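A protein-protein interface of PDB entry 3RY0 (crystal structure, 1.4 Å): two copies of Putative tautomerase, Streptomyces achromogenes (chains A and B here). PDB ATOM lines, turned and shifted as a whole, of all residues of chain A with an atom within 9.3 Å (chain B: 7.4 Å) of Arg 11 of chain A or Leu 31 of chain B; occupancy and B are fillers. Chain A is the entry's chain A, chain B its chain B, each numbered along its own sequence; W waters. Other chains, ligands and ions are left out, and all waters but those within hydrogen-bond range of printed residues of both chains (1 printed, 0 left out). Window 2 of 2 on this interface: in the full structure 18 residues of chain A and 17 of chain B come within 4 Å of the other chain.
NH1 of Arg 11 of chain A lies within hydrogen-bond range of O of Leu 31 of chain B (2.8 Å).
Among the printed residues, merely in contact across the chains: Thr 6 of chain A with Pro 1 of chain B, Leu 7 of chain A with Pro 1 of chain B, Leu 7 of chain A with Leu 31 of chain B, Glu 15 of chain A with Thr 30 of chain B, Ala 18 of chain A with Thr 30 of chain B, Leu 19 of chain A with Ala 27 of chain B, Leu 19 of chain A with Thr 30 of chain B, Ala 22 of chain A with Ala 26 of chain B, Ala 22 of chain A with Thr 30 of chain B and Leu 23 of chain A with Ala 26 of chain B.
Water W1 lies within hydrogen-bond range of the side-chain carboxylate (OE2) of Glu 15 of chain A (2.8 Å) and the backbone carbonyl oxygen (O) of Thr 30 of chain B (3.1 Å).
No residue of chain B comes within 4 Å of Gly 10 of chain A.
Gln 14 of chain A touches none of the printed residues of chain B.
Printed residues of chain B within 4 Å of Glu 15 of chain A: Thr 30 (3.9 Å).
Of the printed residues of chain B, Leu 23 of chain A touches Ala 26 (3.99 Å).
Glu 43 of chain A touches none of the printed residues of chain B.
Of the printed residues of chain A, Pro 1 of chain B touches Thr 6 (3.7 Å) and Leu 7 (3.9 Å).
Printed residues of chain A within 4 Å of Ala 26 of chain B: Ala 22 and Leu 23.
Leu 31 of chain B touches just these residues of chain A: Leu 7 (3.9 Å) and Arg 11 (2.8 Å).
The nearest residue of chain A that does not touch Leu 31 of chain B is Glu 15 of chain A (4.04 Å).
The nearest printed residue of chain A that does not touch Ala 27 of chain B is Leu 23 of chain A (4.5 Å).
The side-chain hydroxyl (OG1) of Thr 6 of chain A is in hydrogen-bond range of the side-chain carboxylate (OE1) of Glu 43 of chain A (3.2 Å).
The backbone carbonyl oxygen (O) of Ala 26 of chain B sits at hydrogen-bond distance from the side-chain hydroxyl (OG1) of Thr 30 of chain B, 2.8 Å away.
The backbone carbonyl oxygen of Glu 43 of chain A sits at hydrogen-bond distance from the backbone NH of Leu 7 of chain A (2.9 Å).
The backbone NH of Ser 12 of chain A sits at hydrogen-bond distance from the side-chain carboxylate of Glu 15 of chain A.
The backbone NH (N) of Thr 45 of chain A sits at hydrogen-bond distance from the backbone carbonyl oxygen (O) of Leu 7 of chain A, 2.9 Å away.
The guanidinium group (NH1) of Arg 11 of chain A is in salt-bridge range of the side-chain carboxylate (OE2) of Glu 15 of chain A.
No position is printed for both chains.
Of the 11 pairs that touch across the chains among the printed residues, none has its exchanged pair printed and touching as well.
Of the 13 printed residues of chain B, 5 touch a printed residue of chain A.
Hydrophobic or aromatic side chains of chain B within 4 Å of the printed part of chain A: Pro 1, Ala 26 and Leu 31.
Printed residues of chain A that touch a printed residue of chain B: Thr 6, Leu 7, Arg 11, Glu 15, Ala 18, Leu 19, Ala 22 and Leu 23.
Hydrophobic or aromatic side chains of chain A within 4 Å of the printed part of chain B: Leu 7, Leu 19, Ala 22 and Leu 23.
Among the printed residues, 11 pairs touch across the chains.
Among the printed residues, no Asp or Glu carboxylate lies within 4 Å of a Lys or Arg side-chain nitrogen of the other chain.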
ATOM      1  N   VAL A   5     -22.791  28.773 -13.697  1.00  0.00           N
ATOM      2  CA  VAL A   5     -21.730  27.791 -13.569  1.00  0.00           C
ATOM      3  C   VAL A   5     -20.703  28.068 -14.658  1.00  0.00           C
ATOM      4  O   VAL A   5     -21.081  28.262 -15.849  1.00  0.00           O
ATOM      5  CB  VAL A   5     -22.278  26.381 -13.797  1.00  0.00           C
ATOM      6  CG1 VAL A   5     -21.207  25.265 -13.691  1.00  0.00           C
ATOM      7  CG2 VAL A   5     -23.437  26.131 -12.911  1.00  0.00           C
ATOM      8  N   THR A   6     -19.420  28.031 -14.295  1.00  0.00           N
ATOM      9  CA  THR A   6     -18.384  28.125 -15.321  1.00  0.00           C
ATOM     10  C   THR A   6     -17.615  26.772 -15.341  1.00  0.00           C
ATOM     11  O   THR A   6     -17.069  26.391 -14.313  1.00  0.00           O
ATOM     12  CB  THR A   6     -17.424  29.262 -14.918  1.00  0.00           C
ATOM     13  OG1 THR A   6     -18.142  30.496 -14.752  1.00  0.00           O
ATOM     14  CG2 THR A   6     -16.369  29.502 -16.050  1.00  0.00           C
ATOM     15  N   LEU A   7     -17.628  26.153 -16.497  1.00  0.00           N
ATOM     16  CA  LEU A   7     -17.024  24.823 -16.690  1.00  0.00           C
ATOM     17  C   LEU A   7     -16.073  24.850 -17.777  1.00  0.00           C
ATOM     18  O   LEU A   7     -16.276  25.585 -18.699  1.00  0.00           O
ATOM     19  CB  LEU A   7     -18.073  23.791 -17.207  1.00  0.00           C
ATOM     20  CG  LEU A   7     -19.304  23.500 -16.380  1.00  0.00           C
ATOM     21  CD1 LEU A   7     -20.101  22.339 -17.028  1.00  0.00           C
ATOM     22  CD2 LEU A   7     -18.849  23.108 -14.915  1.00  0.00           C
ATOM     23  N   LEU A   8     -15.056  23.988 -17.790  1.00  0.00           N
ATOM     24  CA  LEU A   8     -14.279  23.773 -19.035  1.00  0.00           C
ATOM     25  C   LEU A   8     -15.101  23.145 -20.094  1.00  0.00           C
ATOM     26  O   LEU A   8     -15.951  22.226 -19.778  1.00  0.00           O
ATOM     27  CB  LEU A   8     -13.117  22.846 -18.796  1.00  0.00           C
ATOM     28  CG  LEU A   8     -11.973  23.434 -18.056  1.00  0.00           C
ATOM     29  CD1 LEU A   8     -11.021  22.280 -17.517  1.00  0.00           C
ATOM     30  CD2 LEU A   8     -11.123  24.353 -18.970  1.00  0.00           C
ATOM     31  N   GLU A   9     -14.825  23.507 -21.341  1.00  0.00           N
ATOM     32  CA  GLU A   9     -15.331  22.804 -22.512  1.00  0.00           C
ATOM     33  C   GLU A   9     -15.074  21.303 -22.420  1.00  0.00           C
ATOM     34  O   GLU A   9     -14.127  20.826 -21.834  1.00  0.00           O
ATOM     35  CB  GLU A   9     -14.719  23.387 -23.840  1.00  0.00           C
ATOM     36  CG  GLU A   9     -15.296  24.700 -24.266  1.00  0.00           C
ATOM     37  CD  GLU A   9     -14.685  25.281 -25.540  1.00  0.00           C
ATOM     38  OE1 GLU A   9     -13.691  24.708 -26.066  1.00  0.00           O
ATOM     39  OE2 GLU A   9     -15.145  26.318 -26.005  1.00  0.00           O
ATOM     40  N   GLY A  10     -16.006  20.616 -23.062  1.00  0.00           N
ATOM     41  CA  GLY A  10     -15.849  19.222 -23.354  1.00  0.00           C
ATOM     42  C   GLY A  10     -16.758  18.325 -22.532  1.00  0.00           C
ATOM     43  O   GLY A  10     -16.529  17.097 -22.550  1.00  0.00           O
ATOM     44  N   ARG A  11     -17.731  18.858 -21.769  1.00  0.00           N
ATOM     45  CA  ARG A  11     -18.623  17.936 -20.999  1.00  0.00           C
ATOM     46  C   ARG A  11     -19.659  17.457 -21.942  1.00  0.00           C
ATOM     47  O   ARG A  11     -20.032  18.145 -22.906  1.00  0.00           O
ATOM     48  CB  ARG A  11     -19.431  18.632 -19.905  1.00  0.00           C
ATOM     49  CG  ARG A  11     -18.774  18.963 -18.679  1.00  0.00           C
ATOM     50  CD  ARG A  11     -18.299  17.757 -18.085  1.00  0.00           C
ATOM     51  NE  ARG A  11     -17.293  18.039 -17.122  1.00  0.00           N
ATOM     52  CZ  ARG A  11     -16.856  17.156 -16.247  1.00  0.00           C
ATOM     53  NH1 ARG A  11     -17.356  15.911 -16.255  1.00  0.00           N
ATOM     54  NH2 ARG A  11     -15.890  17.489 -15.392  1.00  0.00           N
ATOM     55  N   SER A  12     -20.223  16.277 -21.684  1.00  0.00           N
ATOM     56  CA  SER A  12     -21.220  15.827 -22.590  1.00  0.00           C
ATOM     57  C   SER A  12     -22.531  16.575 -22.390  1.00  0.00           C
ATOM     58  O   SER A  12     -22.801  17.124 -21.260  1.00  0.00           O
ATOM     59  CB  SER A  12     -21.530  14.316 -22.364  1.00  0.00           C
ATOM     60  OG  SER A  12     -21.993  14.072 -21.026  1.00  0.00           O
ATOM     61  N   PRO A  13     -23.366  16.546 -23.398  1.00  0.00           N
ATOM     62  CA  PRO A  13     -24.694  17.127 -23.240  1.00  0.00           C
ATOM     63  C   PRO A  13     -25.456  16.477 -22.075  1.00  0.00           C
ATOM     64  O   PRO A  13     -26.212  17.132 -21.334  1.00  0.00           O
ATOM     65  CB  PRO A  13     -25.370  16.877 -24.576  1.00  0.00           C
ATOM     66  CG  PRO A  13     -24.223  16.853 -25.564  1.00  0.00           C
ATOM     67  CD  PRO A  13     -23.069  16.230 -24.826  1.00  0.00           C
ATOM     68  N   GLN A  14     -25.251  15.188 -21.842  1.00  0.00           N
ATOM     69  CA  GLN A  14     -26.047  14.526 -20.823  1.00  0.00           C
ATOM     70  C   GLN A  14     -25.578  14.999 -19.437  1.00  0.00           C
ATOM     71  O   GLN A  14     -26.365  15.160 -18.526  1.00  0.00           O
ATOM     72  CB  GLN A  14     -25.758  12.989 -20.945  1.00  0.00           C
ATOM     73  CG  GLN A  14     -26.255  12.270 -22.230  1.00  0.00           C
ATOM     74  CD  GLN A  14     -25.665  12.748 -23.622  1.00  0.00           C
ATOM     75  OE1 GLN A  14     -24.482  13.170 -23.761  1.00  0.00           O
ATOM     76  NE2 GLN A  14     -26.524  12.631 -24.680  1.00  0.00           N
ATOM     77  N   GLU A  15     -24.259  15.169 -19.256  1.00  0.00           N
ATOM     78  CA  GLU A  15     -23.730  15.628 -17.996  1.00  0.00           C
ATOM     79  C   GLU A  15     -24.240  17.079 -17.734  1.00  0.00           C
ATOM     80  O   GLU A  15     -24.587  17.369 -16.592  1.00  0.00           O
ATOM     81  CB  GLU A  15     -22.191  15.714 -18.014  1.00  0.00           C
ATOM     82  CG  GLU A  15     -21.510  14.357 -17.974  1.00  0.00           C
ATOM     83  CD  GLU A  15     -20.014  14.484 -18.187  1.00  0.00           C
ATOM     84  OE1 GLU A  15     -19.637  14.938 -19.300  1.00  0.00           O
ATOM     85  OE2 GLU A  15     -19.252  14.126 -17.297  1.00  0.00           O
ATOM     86  N   VAL A  16     -24.224  17.926 -18.770  1.00  0.00           N
ATOM     87  CA  VAL A  16     -24.672  19.356 -18.555  1.00  0.00           C
ATOM     88  C   VAL A  16     -26.154  19.333 -18.164  1.00  0.00           C
ATOM     89  O   VAL A  16     -26.517  20.040 -17.228  1.00  0.00           O
ATOM     90  CB  VAL A  16     -24.423  20.152 -19.803  1.00  0.00           C
ATOM     91  CG1 VAL A  16     -25.101  21.530 -19.639  1.00  0.00           C
ATOM     92  CG2 VAL A  16     -22.888  20.399 -19.945  1.00  0.00           C
ATOM     93  N   ALA A  17     -27.004  18.499 -18.813  1.00  0.00           N
ATOM     94  CA  ALA A  17     -28.409  18.470 -18.462  1.00  0.00           C
ATOM     95  C   ALA A  17     -28.620  17.936 -16.996  1.00  0.00           C
ATOM     96  O   ALA A  17     -29.409  18.439 -16.224  1.00  0.00           O
ATOM     97  CB  ALA A  17     -29.135  17.554 -19.428  1.00  0.00           C
ATOM     98  N   ALA A  18     -27.836  16.925 -16.628  1.00  0.00           N
ATOM     99  CA  ALA A  18     -27.920  16.397 -15.280  1.00  0.00           C
ATOM    100  C   ALA A  18     -27.446  17.402 -14.247  1.00  0.00           C
ATOM    101  O   ALA A  18     -28.052  17.527 -13.171  1.00  0.00           O
ATOM    102  CB  ALA A  18     -27.132  15.119 -15.135  1.00  0.00           C
ATOM    103  N   LEU A  19     -26.389  18.172 -14.563  1.00  0.00           N
ATOM    104  CA  LEU A  19     -25.937  19.234 -13.644  1.00  0.00           C
ATOM    105  C   LEU A  19     -27.031  20.303 -13.398  1.00  0.00           C
ATOM    106  O   LEU A  19     -27.220  20.726 -12.278  1.00  0.00           O
ATOM    107  CB  LEU A  19     -24.671  19.807 -14.295  1.00  0.00           C
ATOM    108  CG  LEU A  19     -24.082  20.976 -13.491  1.00  0.00           C
ATOM    109  CD1 LEU A  19     -23.439  20.553 -12.160  1.00  0.00           C
ATOM    110  CD2 LEU A  19     -23.084  21.771 -14.346  1.00  0.00           C
ATOM    111  N   GLY A  20     -27.667  20.748 -14.500  1.00  0.00           N
ATOM    112  CA  GLY A  20     -28.707  21.742 -14.334  1.00  0.00           C
ATOM    113  C   GLY A  20     -29.798  21.272 -13.382  1.00  0.00           C
ATOM    114  O   GLY A  20     -30.280  22.016 -12.561  1.00  0.00           O
ATOM    115  N   ALA A  22     -29.548  18.859 -11.061  1.00  0.00           N
ATOM    116  CA  ALA A  22     -29.081  18.625  -9.719  1.00  0.00           C
ATOM    117  C   ALA A  22     -28.757  19.848  -8.911  1.00  0.00           C
ATOM    118  O   ALA A  22     -29.035  19.965  -7.711  1.00  0.00           O
ATOM    119  CB  ALA A  22     -27.872  17.695  -9.771  1.00  0.00           C
ATOM    120  N   LEU A  23     -28.252  20.887  -9.618  1.00  0.00           N
ATOM    121  CA  LEU A  23     -28.050  22.182  -8.915  1.00  0.00           C
ATOM    122  C   LEU A  23     -29.372  22.819  -8.497  1.00  0.00           C
ATOM    123  O   LEU A  23     -29.492  23.376  -7.422  1.00  0.00           O
ATOM    124  CB  LEU A  23     -27.260  23.137  -9.836  1.00  0.00           C
ATOM    125  CG  LEU A  23     -25.821  22.708 -10.105  1.00  0.00           C
ATOM    126  CD1 LEU A  23     -25.247  23.695 -11.159  1.00  0.00           C
ATOM    127  CD2 LEU A  23     -24.951  22.788  -8.868  1.00  0.00           C
ATOM    128  N   VAL A  42     -25.212  27.819 -17.718  1.00  0.00           N
ATOM    129  CA  VAL A  42     -23.952  27.061 -17.765  1.00  0.00           C
ATOM    130  C   VAL A  42     -23.108  27.681 -18.836  1.00  0.00           C
ATOM    131  O   VAL A  42     -23.518  27.683 -20.033  1.00  0.00           O
ATOM    132  CB  VAL A  42     -24.174  25.557 -18.020  1.00  0.00           C
ATOM    133  CG1 VAL A  42     -22.798  24.807 -18.173  1.00  0.00           C
ATOM    134  CG2 VAL A  42     -24.931  24.890 -16.916  1.00  0.00           C
ATOM    135  N   GLU A  43     -21.906  28.144 -18.472  1.00  0.00           N
ATOM    136  CA  GLU A  43     -20.992  28.761 -19.459  1.00  0.00           C
ATOM    137  C   GLU A  43     -19.796  27.782 -19.585  1.00  0.00           C
ATOM    138  O   GLU A  43     -19.385  27.149 -18.589  1.00  0.00           O
ATOM    139  CB  GLU A  43     -20.442  30.016 -18.811  1.00  0.00           C
ATOM    140  CG  GLU A  43     -21.472  31.033 -18.496  1.00  0.00           C
ATOM    141  CD  GLU A  43     -20.843  32.244 -17.807  1.00  0.00           C
ATOM    142  OE1 GLU A  43     -19.818  32.086 -17.037  1.00  0.00           O
ATOM    143  OE2 GLU A  43     -21.418  33.335 -18.050  1.00  0.00           O
ATOM    144  N   GLU A  44     -19.277  27.593 -20.800  1.00  0.00           N
ATOM    145  CA  GLU A  44     -18.164  26.668 -21.087  1.00  0.00           C
ATOM    146  C   GLU A  44     -17.018  27.576 -21.553  1.00  0.00           C
ATOM    147  O   GLU A  44     -17.172  28.514 -22.375  1.00  0.00           O
ATOM    148  CB  GLU A  44     -18.555  25.660 -22.171  1.00  0.00           C
ATOM    149  CG  GLU A  44     -19.589  24.709 -21.612  1.00  0.00           C
ATOM    150  CD  GLU A  44     -19.802  23.410 -22.430  1.00  0.00           C
ATOM    151  OE1 GLU A  44     -18.974  23.096 -23.311  1.00  0.00           O
ATOM    152  OE2 GLU A  44     -20.786  22.698 -22.139  1.00  0.00           O
ATOM    153  N   THR A  45     -15.843  27.321 -20.995  1.00  0.00           N
ATOM    154  CA  THR A  45     -14.661  28.073 -21.282  1.00  0.00           C
ATOM    155  C   THR A  45     -13.636  27.131 -21.963  1.00  0.00           C
ATOM    156  O   THR A  45     -13.372  26.037 -21.433  1.00  0.00           O
ATOM    157  CB  THR A  45     -14.040  28.606 -19.954  1.00  0.00           C
ATOM    158  OG1 THR A  45     -15.063  29.435 -19.315  1.00  0.00           O
ATOM    159  CG2 THR A  45     -12.817  29.358 -20.214  1.00  0.00           C
ATOM    160  N   ARG A  61      -2.095  20.742 -18.981  1.00  0.00           N
ATOM    161  CA  ARG A  61      -2.393  19.427 -19.550  1.00  0.00           C
ATOM    162  C   ARG A  61      -1.207  18.969 -20.384  1.00  0.00           C
ATOM    163  O   ARG A  61      -0.859  17.763 -20.376  1.00  0.00           O
ATOM    164  CB  ARG A  61      -3.627  19.511 -20.422  1.00  0.00           C
ATOM    165  CG  ARG A  61      -4.793  19.220 -19.604  1.00  0.00           C
ATOM    166  CD  ARG A  61      -6.044  19.603 -20.358  1.00  0.00           C
ATOM    167  NE  ARG A  61      -7.199  19.246 -19.550  1.00  0.00           N
ATOM    168  CZ  ARG A  61      -8.445  19.531 -19.871  1.00  0.00           C
ATOM    169  NH1 ARG A  61      -8.675  20.205 -20.988  1.00  0.00           N
ATOM    170  NH2 ARG A  61      -9.433  19.114 -19.102  1.00  0.00           N
ATOM    171  N   PRO B   1     -14.744  23.287 -11.208  1.00  0.00           N
ATOM    172  CA  PRO B   1     -15.928  23.931 -11.724  1.00  0.00           C
ATOM    173  C   PRO B   1     -16.197  25.137 -10.810  1.00  0.00           C
ATOM    174  O   PRO B   1     -15.888  25.019  -9.616  1.00  0.00           O
ATOM    175  CB  PRO B   1     -16.956  22.791 -11.514  1.00  0.00           C
ATOM    176  CG  PRO B   1     -16.148  21.590 -11.802  1.00  0.00           C
ATOM    177  CD  PRO B   1     -14.844  21.816 -11.281  1.00  0.00           C
ATOM    178  N   ILE B   3     -18.964  28.009  -9.374  1.00  0.00           N
ATOM    179  CA  ILE B   3     -20.424  28.211  -9.293  1.00  0.00           C
ATOM    180  C   ILE B   3     -20.644  29.522  -8.544  1.00  0.00           C
ATOM    181  O   ILE B   3     -20.130  29.718  -7.406  1.00  0.00           O
ATOM    182  CB  ILE B   3     -21.116  27.031  -8.548  1.00  0.00           C
ATOM    183  CG1 ILE B   3     -20.915  25.755  -9.299  1.00  0.00           C
ATOM    184  CG2 ILE B   3     -22.654  27.373  -8.478  1.00  0.00           C
ATOM    185  CD1 ILE B   3     -21.328  24.495  -8.487  1.00  0.00           C
ATOM    186  N   ALA B  25     -22.024  18.940  -3.686  1.00  0.00           N
ATOM    187  CA  ALA B  25     -22.417  17.566  -3.950  1.00  0.00           C
ATOM    188  C   ALA B  25     -23.029  17.350  -5.293  1.00  0.00           C
ATOM    189  O   ALA B  25     -22.666  16.342  -6.003  1.00  0.00           O
ATOM    190  CB  ALA B  25     -23.390  17.069  -2.809  1.00  0.00           C
ATOM    191  N   ALA B  26     -23.879  18.242  -5.745  1.00  0.00           N
ATOM    192  CA  ALA B  26     -24.521  18.087  -7.058  1.00  0.00           C
ATOM    193  C   ALA B  26     -23.482  18.079  -8.212  1.00  0.00           C
ATOM    194  O   ALA B  26     -23.588  17.299  -9.155  1.00  0.00           O
ATOM    195  CB  ALA B  26     -25.551  19.207  -7.217  1.00  0.00           C
ATOM    196  N   ALA B  27     -22.526  19.056  -8.140  1.00  0.00           N
ATOM    197  CA  ALA B  27     -21.458  19.039  -9.150  1.00  0.00           C
ATOM    198  C   ALA B  27     -20.561  17.779  -9.131  1.00  0.00           C
ATOM    199  O   ALA B  27     -20.311  17.190 -10.171  1.00  0.00           O
ATOM    200  CB  ALA B  27     -20.589  20.341  -8.988  1.00  0.00           C
ATOM    201  N   HIS B  28     -20.245  17.349  -7.912  1.00  0.00           N
ATOM    202  CA  HIS B  28     -19.467  16.110  -7.759  1.00  0.00           C
ATOM    203  C   HIS B  28     -20.196  14.873  -8.326  1.00  0.00           C
ATOM    204  O   HIS B  28     -19.615  14.067  -9.137  1.00  0.00           O
ATOM    205  CB  HIS B  28     -19.127  15.975  -6.293  1.00  0.00           C
ATOM    206  CG  HIS B  28     -18.550  14.655  -5.944  1.00  0.00           C
ATOM    207  ND1 HIS B  28     -17.284  14.274  -6.320  1.00  0.00           N
ATOM    208  CD2 HIS B  28     -18.994  13.721  -5.064  1.00  0.00           C
ATOM    209  CE1 HIS B  28     -17.029  13.092  -5.787  1.00  0.00           C
ATOM    210  NE2 HIS B  28     -18.028  12.761  -4.999  1.00  0.00           N
ATOM    211  N   GLU B  29     -21.484  14.756  -8.016  1.00  0.00           N
ATOM    212  CA  GLU B  29     -22.264  13.626  -8.461  1.00  0.00           C
ATOM    213  C   GLU B  29     -22.389  13.592  -9.970  1.00  0.00           C
ATOM    214  O   GLU B  29     -22.283  12.551 -10.616  1.00  0.00           O
ATOM    215  CB  GLU B  29     -23.661  13.710  -7.763  1.00  0.00           C
ATOM    216  CG  GLU B  29     -23.654  13.185  -6.380  1.00  0.00           C
ATOM    217  CD  GLU B  29     -23.075  11.739  -6.335  1.00  0.00           C
ATOM    218  OE1 GLU B  29     -23.517  10.849  -7.118  1.00  0.00           O
ATOM    219  OE2 GLU B  29     -22.104  11.596  -5.546  1.00  0.00           O
ATOM    220  N   THR B  30     -22.735  14.751 -10.597  1.00  0.00           N
ATOM    221  CA  THR B  30     -23.096  14.788 -11.999  1.00  0.00           C
ATOM    222  C   THR B  30     -21.941  14.912 -12.964  1.00  0.00           C
ATOM    223  O   THR B  30     -22.032  14.441 -14.083  1.00  0.00           O
ATOM    224  CB  THR B  30     -24.136  15.899 -12.304  1.00  0.00           C
ATOM    225  OG1 THR B  30     -23.620  17.190 -11.953  1.00  0.00           O
ATOM    226  CG2 THR B  30     -25.381  15.642 -11.548  1.00  0.00           C
ATOM    227  N   LEU B  31     -20.862  15.523 -12.502  1.00  0.00           N
ATOM    228  CA  LEU B  31     -19.668  15.713 -13.377  1.00  0.00           C
ATOM    229  C   LEU B  31     -18.530  14.767 -12.982  1.00  0.00           C
ATOM    230  O   LEU B  31     -17.530  14.707 -13.688  1.00  0.00           O
ATOM    231  CB  LEU B  31     -19.188  17.155 -13.205  1.00  0.00           C
ATOM    232  CG  LEU B  31     -20.196  18.277 -13.523  1.00  0.00           C
ATOM    233  CD1 LEU B  31     -19.529  19.666 -13.280  1.00  0.00           C
ATOM    234  CD2 LEU B  31     -20.635  18.127 -14.997  1.00  0.00           C
ATOM    235  N   GLY B  32     -18.559  14.144 -11.811  1.00  0.00           N
ATOM    236  CA  GLY B  32     -17.381  13.332 -11.376  1.00  0.00           C
ATOM    237  C   GLY B  32     -16.263  14.196 -10.819  1.00  0.00           C
ATOM    238  O   GLY B  32     -15.128  13.696 -10.615  1.00  0.00           O
ATOM    239  N   THR B  33     -16.485  15.466 -10.595  1.00  0.00           N
ATOM    240  CA  THR B  33     -15.438  16.433 -10.155  1.00  0.00           C
ATOM    241  C   THR B  33     -15.148  16.068  -8.726  1.00  0.00           C
ATOM    242  O   THR B  33     -16.073  15.958  -7.939  1.00  0.00           O
ATOM    243  CB  THR B  33     -16.105  17.879 -10.092  1.00  0.00           C
ATOM    244  OG1 THR B  33     -16.692  18.250 -11.343  1.00  0.00           O
ATOM    245  CG2 THR B  33     -15.019  18.976  -9.659  1.00  0.00           C
ATOM    246  N   PRO B  34     -13.871  15.962  -8.334  1.00  0.00           N
ATOM    247  CA  PRO B  34     -13.540  15.863  -6.914  1.00  0.00           C
ATOM    248  C   PRO B  34     -14.144  17.042  -6.105  1.00  0.00           C
ATOM    249  O   PRO B  34     -14.237  18.207  -6.658  1.00  0.00           O
ATOM    250  CB  PRO B  34     -11.961  15.832  -6.914  1.00  0.00           C
ATOM    251  CG  PRO B  34     -11.663  15.360  -8.298  1.00  0.00           C
ATOM    252  CD  PRO B  34     -12.679  15.961  -9.204  1.00  0.00           C
ATOM    253  N   VAL B  38     -14.499  21.872  -6.614  1.00  0.00           N
ATOM    254  CA  VAL B  38     -15.733  22.672  -6.816  1.00  0.00           C
ATOM    255  C   VAL B  38     -15.595  23.889  -5.924  1.00  0.00           C
ATOM    256  O   VAL B  38     -15.383  23.794  -4.715  1.00  0.00           O
ATOM    257  CB  VAL B  38     -17.003  21.903  -6.436  1.00  0.00           C
ATOM    258  CG1 VAL B  38     -18.183  22.793  -6.752  1.00  0.00           C
ATOM    259  CG2 VAL B  38     -17.094  20.561  -7.290  1.00  0.00           C
HETATM  260  O   HOH W   1     -19.982  12.435 -15.221  1.00  0.00           O
